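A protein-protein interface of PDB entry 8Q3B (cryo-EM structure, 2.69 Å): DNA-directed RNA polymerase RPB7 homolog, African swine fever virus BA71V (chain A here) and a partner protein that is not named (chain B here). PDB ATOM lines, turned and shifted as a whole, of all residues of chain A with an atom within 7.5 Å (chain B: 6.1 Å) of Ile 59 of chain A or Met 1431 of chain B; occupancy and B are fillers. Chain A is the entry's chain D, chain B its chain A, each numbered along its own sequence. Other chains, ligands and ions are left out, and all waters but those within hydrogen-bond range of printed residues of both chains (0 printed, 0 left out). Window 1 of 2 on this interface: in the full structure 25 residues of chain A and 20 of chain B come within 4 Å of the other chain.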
ATOM      1  N   ILE A  13     -13.342  20.522  21.343  1.00  0.00           N
ATOM      2  CA  ILE A  13     -14.420  19.557  21.170  1.00  0.00           C
ATOM      3  C   ILE A  13     -15.616  20.061  21.962  1.00  0.00           C
ATOM      4  O   ILE A  13     -15.555  20.158  23.196  1.00  0.00           O
ATOM      5  CB  ILE A  13     -14.002  18.153  21.634  1.00  0.00           C
ATOM      6  CG1 ILE A  13     -12.800  17.662  20.825  1.00  0.00           C
ATOM      7  CG2 ILE A  13     -15.154  17.175  21.488  1.00  0.00           C
ATOM      8  CD1 ILE A  13     -11.895  16.736  21.593  1.00  0.00           C
ATOM      9  N   ASP A  15     -18.722  18.663  22.125  1.00  0.00           N
ATOM     10  CA  ASP A  15     -19.508  17.575  22.707  1.00  0.00           C
ATOM     11  C   ASP A  15     -18.588  16.382  22.913  1.00  0.00           C
ATOM     12  O   ASP A  15     -18.585  15.437  22.112  1.00  0.00           O
ATOM     13  CB  ASP A  15     -20.696  17.216  21.812  1.00  0.00           C
ATOM     14  CG  ASP A  15     -21.581  16.148  22.421  1.00  0.00           C
ATOM     15  OD1 ASP A  15     -21.365  15.794  23.599  1.00  0.00           O
ATOM     16  OD2 ASP A  15     -22.499  15.667  21.724  1.00  0.00           O
ATOM     17  N   PRO A  16     -17.784  16.392  23.981  1.00  0.00           N
ATOM     18  CA  PRO A  16     -16.819  15.294  24.172  1.00  0.00           C
ATOM     19  C   PRO A  16     -17.464  13.921  24.244  1.00  0.00           C
ATOM     20  O   PRO A  16     -16.892  12.947  23.739  1.00  0.00           O
ATOM     21  CB  PRO A  16     -16.127  15.666  25.490  1.00  0.00           C
ATOM     22  CG  PRO A  16     -16.354  17.129  25.652  1.00  0.00           C
ATOM     23  CD  PRO A  16     -17.688  17.403  25.045  1.00  0.00           C
ATOM     24  N   THR A  17     -18.643  13.812  24.861  1.00  0.00           N
ATOM     25  CA  THR A  17     -19.280  12.506  24.999  1.00  0.00           C
ATOM     26  C   THR A  17     -19.580  11.895  23.637  1.00  0.00           C
ATOM     27  O   THR A  17     -19.321  10.708  23.411  1.00  0.00           O
ATOM     28  CB  THR A  17     -20.563  12.633  25.822  1.00  0.00           C
ATOM     29  OG1 THR A  17     -20.266  13.238  27.086  1.00  0.00           O
ATOM     30  CG2 THR A  17     -21.188  11.266  26.057  1.00  0.00           C
ATOM     31  N   ASN A  18     -20.128  12.690  22.718  1.00  0.00           N
ATOM     32  CA  ASN A  18     -20.377  12.193  21.370  1.00  0.00           C
ATOM     33  C   ASN A  18     -19.084  12.047  20.581  1.00  0.00           C
ATOM     34  O   ASN A  18     -18.960  11.135  19.757  1.00  0.00           O
ATOM     35  CB  ASN A  18     -21.336  13.126  20.636  1.00  0.00           C
ATOM     36  CG  ASN A  18     -21.487  12.771  19.172  1.00  0.00           C
ATOM     37  OD1 ASN A  18     -21.482  11.597  18.803  1.00  0.00           O
ATOM     38  ND2 ASN A  18     -21.620  13.786  18.328  1.00  0.00           N
ATOM     39  N   PHE A  19     -18.114  12.932  20.817  1.00  0.00           N
ATOM     40  CA  PHE A  19     -16.861  12.874  20.074  1.00  0.00           C
ATOM     41  C   PHE A  19     -16.119  11.572  20.345  1.00  0.00           C
ATOM     42  O   PHE A  19     -15.567  10.960  19.423  1.00  0.00           O
ATOM     43  CB  PHE A  19     -15.985  14.072  20.434  1.00  0.00           C
ATOM     44  CG  PHE A  19     -14.669  14.102  19.711  1.00  0.00           C
ATOM     45  CD1 PHE A  19     -14.551  14.738  18.488  1.00  0.00           C
ATOM     46  CD2 PHE A  19     -13.550  13.498  20.255  1.00  0.00           C
ATOM     47  CE1 PHE A  19     -13.344  14.768  17.823  1.00  0.00           C
ATOM     48  CE2 PHE A  19     -12.341  13.525  19.591  1.00  0.00           C
ATOM     49  CZ  PHE A  19     -12.239  14.160  18.376  1.00  0.00           C
ATOM     50  N   CYS A  20     -16.095  11.131  21.603  1.00  0.00           N
ATOM     51  CA  CYS A  20     -15.288   9.976  21.978  1.00  0.00           C
ATOM     52  C   CYS A  20     -15.857   8.654  21.481  1.00  0.00           C
ATOM     53  O   CYS A  20     -15.177   7.630  21.600  1.00  0.00           O
ATOM     54  CB  CYS A  20     -15.129   9.920  23.496  1.00  0.00           C
ATOM     55  SG  CYS A  20     -13.868  11.036  24.137  1.00  0.00           S
ATOM     56  N   PRO A  56      -5.231  12.404  25.257  1.00  0.00           N
ATOM     57  CA  PRO A  56      -6.574  12.160  25.790  1.00  0.00           C
ATOM     58  C   PRO A  56      -7.436  13.409  25.688  1.00  0.00           C
ATOM     59  O   PRO A  56      -6.940  14.537  25.714  1.00  0.00           O
ATOM     60  CB  PRO A  56      -6.317  11.773  27.251  1.00  0.00           C
ATOM     61  CG  PRO A  56      -4.883  11.378  27.309  1.00  0.00           C
ATOM     62  CD  PRO A  56      -4.190  12.202  26.277  1.00  0.00           C
ATOM     63  N   CYS A  57      -8.744  13.197  25.564  1.00  0.00           N
ATOM     64  CA  CYS A  57      -9.671  14.312  25.430  1.00  0.00           C
ATOM     65  C   CYS A  57      -9.821  15.030  26.764  1.00  0.00           C
ATOM     66  O   CYS A  57     -10.725  14.720  27.546  1.00  0.00           O
ATOM     67  CB  CYS A  57     -11.031  13.825  24.929  1.00  0.00           C
ATOM     68  SG  CYS A  57     -12.207  15.151  24.581  1.00  0.00           S
ATOM     69  N   PHE A  58      -8.940  15.990  27.027  1.00  0.00           N
ATOM     70  CA  PHE A  58      -8.974  16.723  28.280  1.00  0.00           C
ATOM     71  C   PHE A  58     -10.244  17.567  28.372  1.00  0.00           C
ATOM     72  O   PHE A  58     -11.005  17.708  27.411  1.00  0.00           O
ATOM     73  CB  PHE A  58      -7.742  17.616  28.407  1.00  0.00           C
ATOM     74  CG  PHE A  58      -6.442  16.868  28.369  1.00  0.00           C
ATOM     75  CD1 PHE A  58      -6.029  16.116  29.454  1.00  0.00           C
ATOM     76  CD2 PHE A  58      -5.631  16.920  27.250  1.00  0.00           C
ATOM     77  CE1 PHE A  58      -4.833  15.429  29.421  1.00  0.00           C
ATOM     78  CE2 PHE A  58      -4.434  16.234  27.214  1.00  0.00           C
ATOM     79  CZ  PHE A  58      -4.035  15.488  28.301  1.00  0.00           C
ATOM     80  N   ILE A  59     -10.467  18.130  29.555  1.00  0.00           N
ATOM     81  CA  ILE A  59     -11.604  19.002  29.827  1.00  0.00           C
ATOM     82  C   ILE A  59     -11.063  20.375  30.201  1.00  0.00           C
ATOM     83  O   ILE A  59     -10.168  20.485  31.048  1.00  0.00           O
ATOM     84  CB  ILE A  59     -12.496  18.440  30.949  1.00  0.00           C
ATOM     85  CG1 ILE A  59     -12.947  17.014  30.618  1.00  0.00           C
ATOM     86  CG2 ILE A  59     -13.702  19.338  31.170  1.00  0.00           C
ATOM     87  CD1 ILE A  59     -13.718  16.883  29.323  1.00  0.00           C
ATOM     88  N   MET A  60     -11.602  21.415  29.570  1.00  0.00           N
ATOM     89  CA  MET A  60     -11.105  22.767  29.790  1.00  0.00           C
ATOM     90  C   MET A  60     -11.299  23.182  31.243  1.00  0.00           C
ATOM     91  O   MET A  60     -12.420  23.169  31.760  1.00  0.00           O
ATOM     92  CB  MET A  60     -11.823  23.742  28.859  1.00  0.00           C
ATOM     93  CG  MET A  60     -11.780  23.344  27.395  1.00  0.00           C
ATOM     94  SD  MET A  60     -12.131  24.721  26.289  1.00  0.00           S
ATOM     95  CE  MET A  60     -12.524  23.849  24.778  1.00  0.00           C
ATOM     96  N   ARG A  61     -10.196  23.552  31.898  1.00  0.00           N
ATOM     97  CA  ARG A  61     -10.265  24.007  33.284  1.00  0.00           C
ATOM     98  C   ARG A  61     -10.750  25.448  33.373  1.00  0.00           C
ATOM     99  O   ARG A  61     -11.629  25.771  34.179  1.00  0.00           O
ATOM    100  CB  ARG A  61      -8.892  23.883  33.942  1.00  0.00           C
ATOM    101  CG  ARG A  61      -8.497  22.483  34.365  1.00  0.00           C
ATOM    102  CD  ARG A  61      -7.272  22.533  35.265  1.00  0.00           C
ATOM    103  NE  ARG A  61      -6.355  23.598  34.867  1.00  0.00           N
ATOM    104  CZ  ARG A  61      -6.191  24.747  35.512  1.00  0.00           C
ATOM    105  NH1 ARG A  61      -6.892  25.046  36.593  1.00  0.00           N
ATOM    106  NH2 ARG A  61      -5.307  25.626  35.051  1.00  0.00           N
ATOM    107  N   THR A  62     -10.182  26.331  32.551  1.00  0.00           N
ATOM    108  CA  THR A  62     -10.348  27.765  32.770  1.00  0.00           C
ATOM    109  C   THR A  62     -11.801  28.197  32.614  1.00  0.00           C
ATOM    110  O   THR A  62     -12.273  29.071  33.350  1.00  0.00           O
ATOM    111  CB  THR A  62      -9.451  28.546  31.813  1.00  0.00           C
ATOM    112  OG1 THR A  62      -9.742  28.165  30.462  1.00  0.00           O
ATOM    113  CG2 THR A  62      -7.985  28.271  32.115  1.00  0.00           C
ATOM    114  N   ASN A  63     -12.519  27.620  31.659  1.00  0.00           N
ATOM    115  CA  ASN A  63     -13.923  27.942  31.457  1.00  0.00           C
ATOM    116  C   ASN A  63     -14.807  26.903  32.136  1.00  0.00           C
ATOM    117  O   ASN A  63     -14.382  25.783  32.427  1.00  0.00           O
ATOM    118  CB  ASN A  63     -14.263  28.032  29.967  1.00  0.00           C
ATOM    119  CG  ASN A  63     -13.731  26.862  29.170  1.00  0.00           C
ATOM    120  OD1 ASN A  63     -14.403  25.843  29.020  1.00  0.00           O
ATOM    121  ND2 ASN A  63     -12.523  27.008  28.645  1.00  0.00           N
ATOM    122  N   SER A  65     -17.527  25.580  30.864  1.00  0.00           N
ATOM    123  CA  SER A  65     -18.198  24.693  29.929  1.00  0.00           C
ATOM    124  C   SER A  65     -17.580  23.303  29.984  1.00  0.00           C
ATOM    125  O   SER A  65     -16.396  23.135  30.288  1.00  0.00           O
ATOM    126  CB  SER A  65     -18.107  25.246  28.508  1.00  0.00           C
ATOM    127  OG  SER A  65     -16.757  25.364  28.100  1.00  0.00           O
ATOM    128  N   GLY A  66     -18.399  22.295  29.684  1.00  0.00           N
ATOM    129  CA  GLY A  66     -17.911  20.930  29.644  1.00  0.00           C
ATOM    130  C   GLY A  66     -17.061  20.608  28.434  1.00  0.00           C
ATOM    131  O   GLY A  66     -16.554  19.487  28.336  1.00  0.00           O
ATOM    132  N   ARG A  67     -16.903  21.561  27.517  1.00  0.00           N
ATOM    133  CA  ARG A  67     -16.114  21.338  26.313  1.00  0.00           C
ATOM    134  C   ARG A  67     -14.728  20.821  26.674  1.00  0.00           C
ATOM    135  O   ARG A  67     -14.198  21.103  27.750  1.00  0.00           O
ATOM    136  CB  ARG A  67     -16.001  22.639  25.515  1.00  0.00           C
ATOM    137  CG  ARG A  67     -17.341  23.243  25.127  1.00  0.00           C
ATOM    138  CD  ARG A  67     -17.196  24.661  24.605  1.00  0.00           C
ATOM    139  NE  ARG A  67     -16.359  24.731  23.411  1.00  0.00           N
ATOM    140  CZ  ARG A  67     -15.305  25.523  23.262  1.00  0.00           C
ATOM    141  NH1 ARG A  67     -14.912  26.350  24.220  1.00  0.00           N
ATOM    142  NH2 ARG A  67     -14.628  25.490  22.119  1.00  0.00           N
ATOM    143  N   GLY A  68     -14.144  20.044  25.760  1.00  0.00           N
ATOM    144  CA  GLY A  68     -12.817  19.502  25.933  1.00  0.00           C
ATOM    145  C   GLY A  68     -11.867  19.991  24.853  1.00  0.00           C
ATOM    146  O   GLY A  68     -12.235  20.770  23.972  1.00  0.00           O
ATOM    147  N   TYR A  69     -10.631  19.507  24.936  1.00  0.00           N
ATOM    148  CA  TYR A  69      -9.640  19.811  23.916  1.00  0.00           C
ATOM    149  C   TYR A  69      -8.722  18.611  23.747  1.00  0.00           C
ATOM    150  O   TYR A  69      -8.551  17.800  24.659  1.00  0.00           O
ATOM    151  CB  TYR A  69      -8.832  21.067  24.260  1.00  0.00           C
ATOM    152  CG  TYR A  69      -8.049  20.972  25.547  1.00  0.00           C
ATOM    153  CD1 TYR A  69      -8.671  21.137  26.774  1.00  0.00           C
ATOM    154  CD2 TYR A  69      -6.685  20.726  25.533  1.00  0.00           C
ATOM    155  CE1 TYR A  69      -7.958  21.055  27.950  1.00  0.00           C
ATOM    156  CE2 TYR A  69      -5.964  20.641  26.704  1.00  0.00           C
ATOM    157  CZ  TYR A  69      -6.606  20.807  27.910  1.00  0.00           C
ATOM    158  OH  TYR A  69      -5.893  20.724  29.082  1.00  0.00           O
ATOM    159  N   MET A  70      -8.133  18.510  22.559  1.00  0.00           N
ATOM    160  CA  MET A  70      -7.289  17.374  22.204  1.00  0.00           C
ATOM    161  C   MET A  70      -6.084  17.877  21.428  1.00  0.00           C
ATOM    162  O   MET A  70      -6.242  18.556  20.411  1.00  0.00           O
ATOM    163  CB  MET A  70      -8.070  16.354  21.371  1.00  0.00           C
ATOM    164  CG  MET A  70      -7.282  15.104  21.021  1.00  0.00           C
ATOM    165  SD  MET A  70      -8.318  13.781  20.371  1.00  0.00           S
ATOM    166  CE  MET A  70      -9.260  13.331  21.825  1.00  0.00           C
ATOM    167  N   TYR B   5      -7.636  25.562  22.517  1.00  0.00           N
ATOM    168  CA  TYR B   5      -7.542  25.907  23.927  1.00  0.00           C
ATOM    169  C   TYR B   5      -6.097  25.819  24.400  1.00  0.00           C
ATOM    170  O   TYR B   5      -5.361  24.900  24.033  1.00  0.00           O
ATOM    171  CB  TYR B   5      -8.434  24.974  24.747  1.00  0.00           C
ATOM    172  CG  TYR B   5      -8.239  25.063  26.240  1.00  0.00           C
ATOM    173  CD1 TYR B   5      -8.979  25.951  27.006  1.00  0.00           C
ATOM    174  CD2 TYR B   5      -7.327  24.244  26.890  1.00  0.00           C
ATOM    175  CE1 TYR B   5      -8.808  26.027  28.371  1.00  0.00           C
ATOM    176  CE2 TYR B   5      -7.150  24.316  28.253  1.00  0.00           C
ATOM    177  CZ  TYR B   5      -7.892  25.207  28.988  1.00  0.00           C
ATOM    178  OH  TYR B   5      -7.715  25.276  30.348  1.00  0.00           O
ATOM    179  N   MET B 472     -21.840  23.677  36.885  1.00  0.00           N
ATOM    180  CA  MET B 472     -20.621  23.345  37.614  1.00  0.00           C
ATOM    181  C   MET B 472     -20.576  24.056  38.960  1.00  0.00           C
ATOM    182  O   MET B 472     -20.263  23.447  39.990  1.00  0.00           O
ATOM    183  CB  MET B 472     -19.397  23.710  36.773  1.00  0.00           C
ATOM    184  CG  MET B 472     -19.154  22.784  35.594  1.00  0.00           C
ATOM    185  SD  MET B 472     -17.416  22.709  35.127  1.00  0.00           S
ATOM    186  CE  MET B 472     -17.534  22.081  33.456  1.00  0.00           C
ATOM    187  N   ILE B1429      -9.240  15.996  34.480  1.00  0.00           N
ATOM    188  CA  ILE B1429     -10.284  15.037  34.147  1.00  0.00           C
ATOM    189  C   ILE B1429     -10.224  14.787  32.649  1.00  0.00           C
ATOM    190  O   ILE B1429     -10.265  15.733  31.856  1.00  0.00           O
ATOM    191  CB  ILE B1429     -11.681  15.541  34.559  1.00  0.00           C
ATOM    192  CG1 ILE B1429     -11.688  15.992  36.021  1.00  0.00           C
ATOM    193  CG2 ILE B1429     -12.723  14.457  34.336  1.00  0.00           C
ATOM    194  CD1 ILE B1429     -11.299  14.911  37.011  1.00  0.00           C
ATOM    195  N   ILE B1430     -10.119  13.519  32.267  1.00  0.00           N
ATOM    196  CA  ILE B1430     -10.089  13.123  30.866  1.00  0.00           C
ATOM    197  C   ILE B1430     -11.224  12.142  30.621  1.00  0.00           C
ATOM    198  O   ILE B1430     -11.655  11.418  31.524  1.00  0.00           O
ATOM    199  CB  ILE B1430      -8.729  12.511  30.468  1.00  0.00           C
ATOM    200  CG1 ILE B1430      -8.551  11.124  31.091  1.00  0.00           C
ATOM    201  CG2 ILE B1430      -7.600  13.432  30.889  1.00  0.00           C
ATOM    202  CD1 ILE B1430      -7.214  10.486  30.791  1.00  0.00           C
ATOM    203  N   MET B1431     -11.708  12.126  29.385  1.00  0.00           N
ATOM    204  CA  MET B1431     -12.859  11.310  29.032  1.00  0.00           C
ATOM    205  C   MET B1431     -12.440   9.857  28.852  1.00  0.00           C
ATOM    206  O   MET B1431     -11.369   9.567  28.310  1.00  0.00           O
ATOM    207  CB  MET B1431     -13.501  11.838  27.751  1.00  0.00           C
ATOM    208  CG  MET B1431     -13.968  13.291  27.844  1.00  0.00           C
ATOM    209  SD  MET B1431     -15.636  13.553  28.488  1.00  0.00           S
ATOM    210  CE  MET B1431     -16.598  12.374  27.550  1.00  0.00           C
ATOM    211  N   ASP B1432     -13.289   8.941  29.314  1.00  0.00           N
ATOM    212  CA  ASP B1432     -13.021   7.508  29.208  1.00  0.00           C
ATOM    213  C   ASP B1432     -13.486   7.036  27.839  1.00  0.00           C
ATOM    214  O   ASP B1432     -14.646   6.678  27.635  1.00  0.00           O
ATOM    215  CB  ASP B1432     -13.716   6.741  30.325  1.00  0.00           C
ATOM    216  CG  ASP B1432     -13.143   5.355  30.523  1.00  0.00           C
ATOM    217  OD1 ASP B1432     -12.410   4.881  29.632  1.00  0.00           O
ATOM    218  OD2 ASP B1432     -13.425   4.740  31.571  1.00  0.00           O
ATOM    219  N   GLU B1433     -12.559   7.036  26.880  1.00  0.00           N
ATOM    220  CA  GLU B1433     -12.903   6.636  25.521  1.00  0.00           C
ATOM    221  C   GLU B1433     -13.302   5.167  25.459  1.00  0.00           C
ATOM    222  O   GLU B1433     -14.256   4.808  24.761  1.00  0.00           O
ATOM    223  CB  GLU B1433     -11.728   6.914  24.585  1.00  0.00           C
ATOM    224  CG  GLU B1433     -11.209   8.343  24.653  1.00  0.00           C
ATOM    225  CD  GLU B1433      -9.829   8.489  24.050  1.00  0.00           C
ATOM    226  OE1 GLU B1433      -9.454   7.643  23.211  1.00  0.00           O
ATOM    227  OE2 GLU B1433      -9.118   9.448  24.414  1.00  0.00           O
ATOM    228  N   LYS B1434     -12.583   4.304  26.180  1.00  0.00           N
ATOM    229  CA  LYS B1434     -12.893   2.878  26.143  1.00  0.00           C
ATOM    230  C   LYS B1434     -14.288   2.603  26.691  1.00  0.00           C
ATOM    231  O   LYS B1434     -15.034   1.792  26.131  1.00  0.00           O
ATOM    232  CB  LYS B1434     -11.844   2.094  26.930  1.00  0.00           C
ATOM    233  CG  LYS B1434     -12.074   0.591  26.953  1.00  0.00           C
ATOM    234  CD  LYS B1434     -11.063  -0.114  27.843  1.00  0.00           C
ATOM    235  CE  LYS B1434     -11.384  -1.593  28.003  1.00  0.00           C
ATOM    236  NZ  LYS B1434     -12.754  -1.829  28.537  1.00  0.00           N
ATOM    237  N   ILE B1436     -16.856   4.746  26.847  1.00  0.00           N
ATOM    238  CA  ILE B1436     -17.892   5.358  26.021  1.00  0.00           C
ATOM    239  C   ILE B1436     -18.093   4.569  24.735  1.00  0.00           C
ATOM    240  O   ILE B1436     -19.231   4.333  24.309  1.00  0.00           O
ATOM    241  CB  ILE B1436     -17.537   6.828  25.737  1.00  0.00           C
ATOM    242  CG1 ILE B1436     -17.579   7.632  27.036  1.00  0.00           C
ATOM    243  CG2 ILE B1436     -18.498   7.429  24.720  1.00  0.00           C
ATOM    244  CD1 ILE B1436     -16.925   8.983  26.941  1.00  0.00           C
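The backbone NH of Phe 58 of chain A sits at hydrogen-bond distance from the backbone carbonyl oxygen of Tyr 69 of chain A (3.0 Å). OD1 of Asn 63 of chain A sits at hydrogen-bond distance from OG of Ser 65 of chain A, at 2.6 Å. ND2 of Asn 63 of chain A is in hydrogen-bond range of SD of Met 60 of chain A (3.3 Å). The side-chain sulfur of Cys 20 of chain A lies close to the backbone carbonyl oxygen of Pro 16 of chain A. The backbone NH (N) of Met 60 of chain A sits at hydrogen-bond distance from the backbone carbonyl oxygen (O) of Arg 67 of chain A (3.2 Å).
Hydrophobic or aromatic side chains of chain B within 4 Å of the printed part of chain A: Tyr 5, Met 472, Ile 1430, Met 1431 and Ile 1436.
N of Met 1431 of chain B is in hydrogen-bond range of O of Cys 57 of chain A (3.3 Å). N of Thr 62 of chain A lies within hydrogen-bond range of OH of Tyr 5 of chain B, 3.5 Å away. The backbone NH (N) of Arg 61 of chain A sits at hydrogen-bond distance from the side-chain hydroxyl (OH) of Tyr 5 of chain B (3.4 Å). The backbone NH (N) of Ile 59 of chain A sits close to the backbone carbonyl oxygen (O) of Ile 1429 of chain B (3.3 Å).
Of the printed residues of chain B, Ile 59 of chain A touches Ile 1429 and Met 1431. Printed residues of chain A within 4 Å of Met 1431 of chain B: Pro 16 (3.7 Å), Thr 17 (3.7 Å), Cys 20 (3.7 Å), Cys 57 (3.3 Å) and Ile 59 (3.9 Å). Printed residues of chain B within 4 Å of Arg 61 of chain A: Tyr 5 (3.4 Å). Printed residues of chain A within 4 Å of Ile 1429 of chain B: Phe 58 (3.9 Å) and Ile 59 (3.2 Å). Of the printed residues of chain B, Tyr 69 of chain A touches Tyr 5. Of the printed residues of chain A, Ile 1436 of chain B touches Thr 17 and Cys 20. Of the printed residues of chain B, Cys 20 of chain A touches Met 1431, Glu 1433 and Ile 1436. Lys 1434 of chain B touches none of the printed residues of chain A. The nearest printed residue of chain B that does not touch Cys 20 of chain A is Asp 1432 of chain B (5.3 Å).
Among the printed residues, merely in contact across the chains: Pro 16 of chain A with Met 1431 of chain B (3.7 Å), Thr 17 of chain A with Met 1431 of chain B (3.7 Å), Thr 17 of chain A with Ile 1436 of chain B (3.6 Å), Cys 20 of chain A with Met 1431 of chain B (3.7 Å), Cys 20 of chain A with Glu 1433 of chain B (3.8 Å), Cys 20 of chain A with Ile 1436 of chain B (3.996 Å), Pro 56 of chain A with Ile 1430 of chain B (3.9 Å), Pro 56 of chain A with Glu 1433 of chain B (3.96 Å), Cys 57 of chain A with Ile 1430 of chain B (3.7 Å), Cys 57 of chain A with Glu 1433 of chain B (3.9 Å), Phe 58 of chain A with Ile 1429 of chain B (3.9 Å), Phe 58 of chain A with Ile 1430 of chain B (3.4 Å), Ile 59 of chain A with Met 1431 of chain B (3.9 Å), Met 60 of chain A with Tyr 5 of chain B (3.5 Å), Asn 63 of chain A with Tyr 5 of chain B (3.9 Å), Ser 65 of chain A with Met 472 of chain B (3.5 Å), Gly 66 of chain A with Met 472 of chain B (3.9 Å) and Tyr 69 of chain A with Tyr 5 of chain B (3.4 Å).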
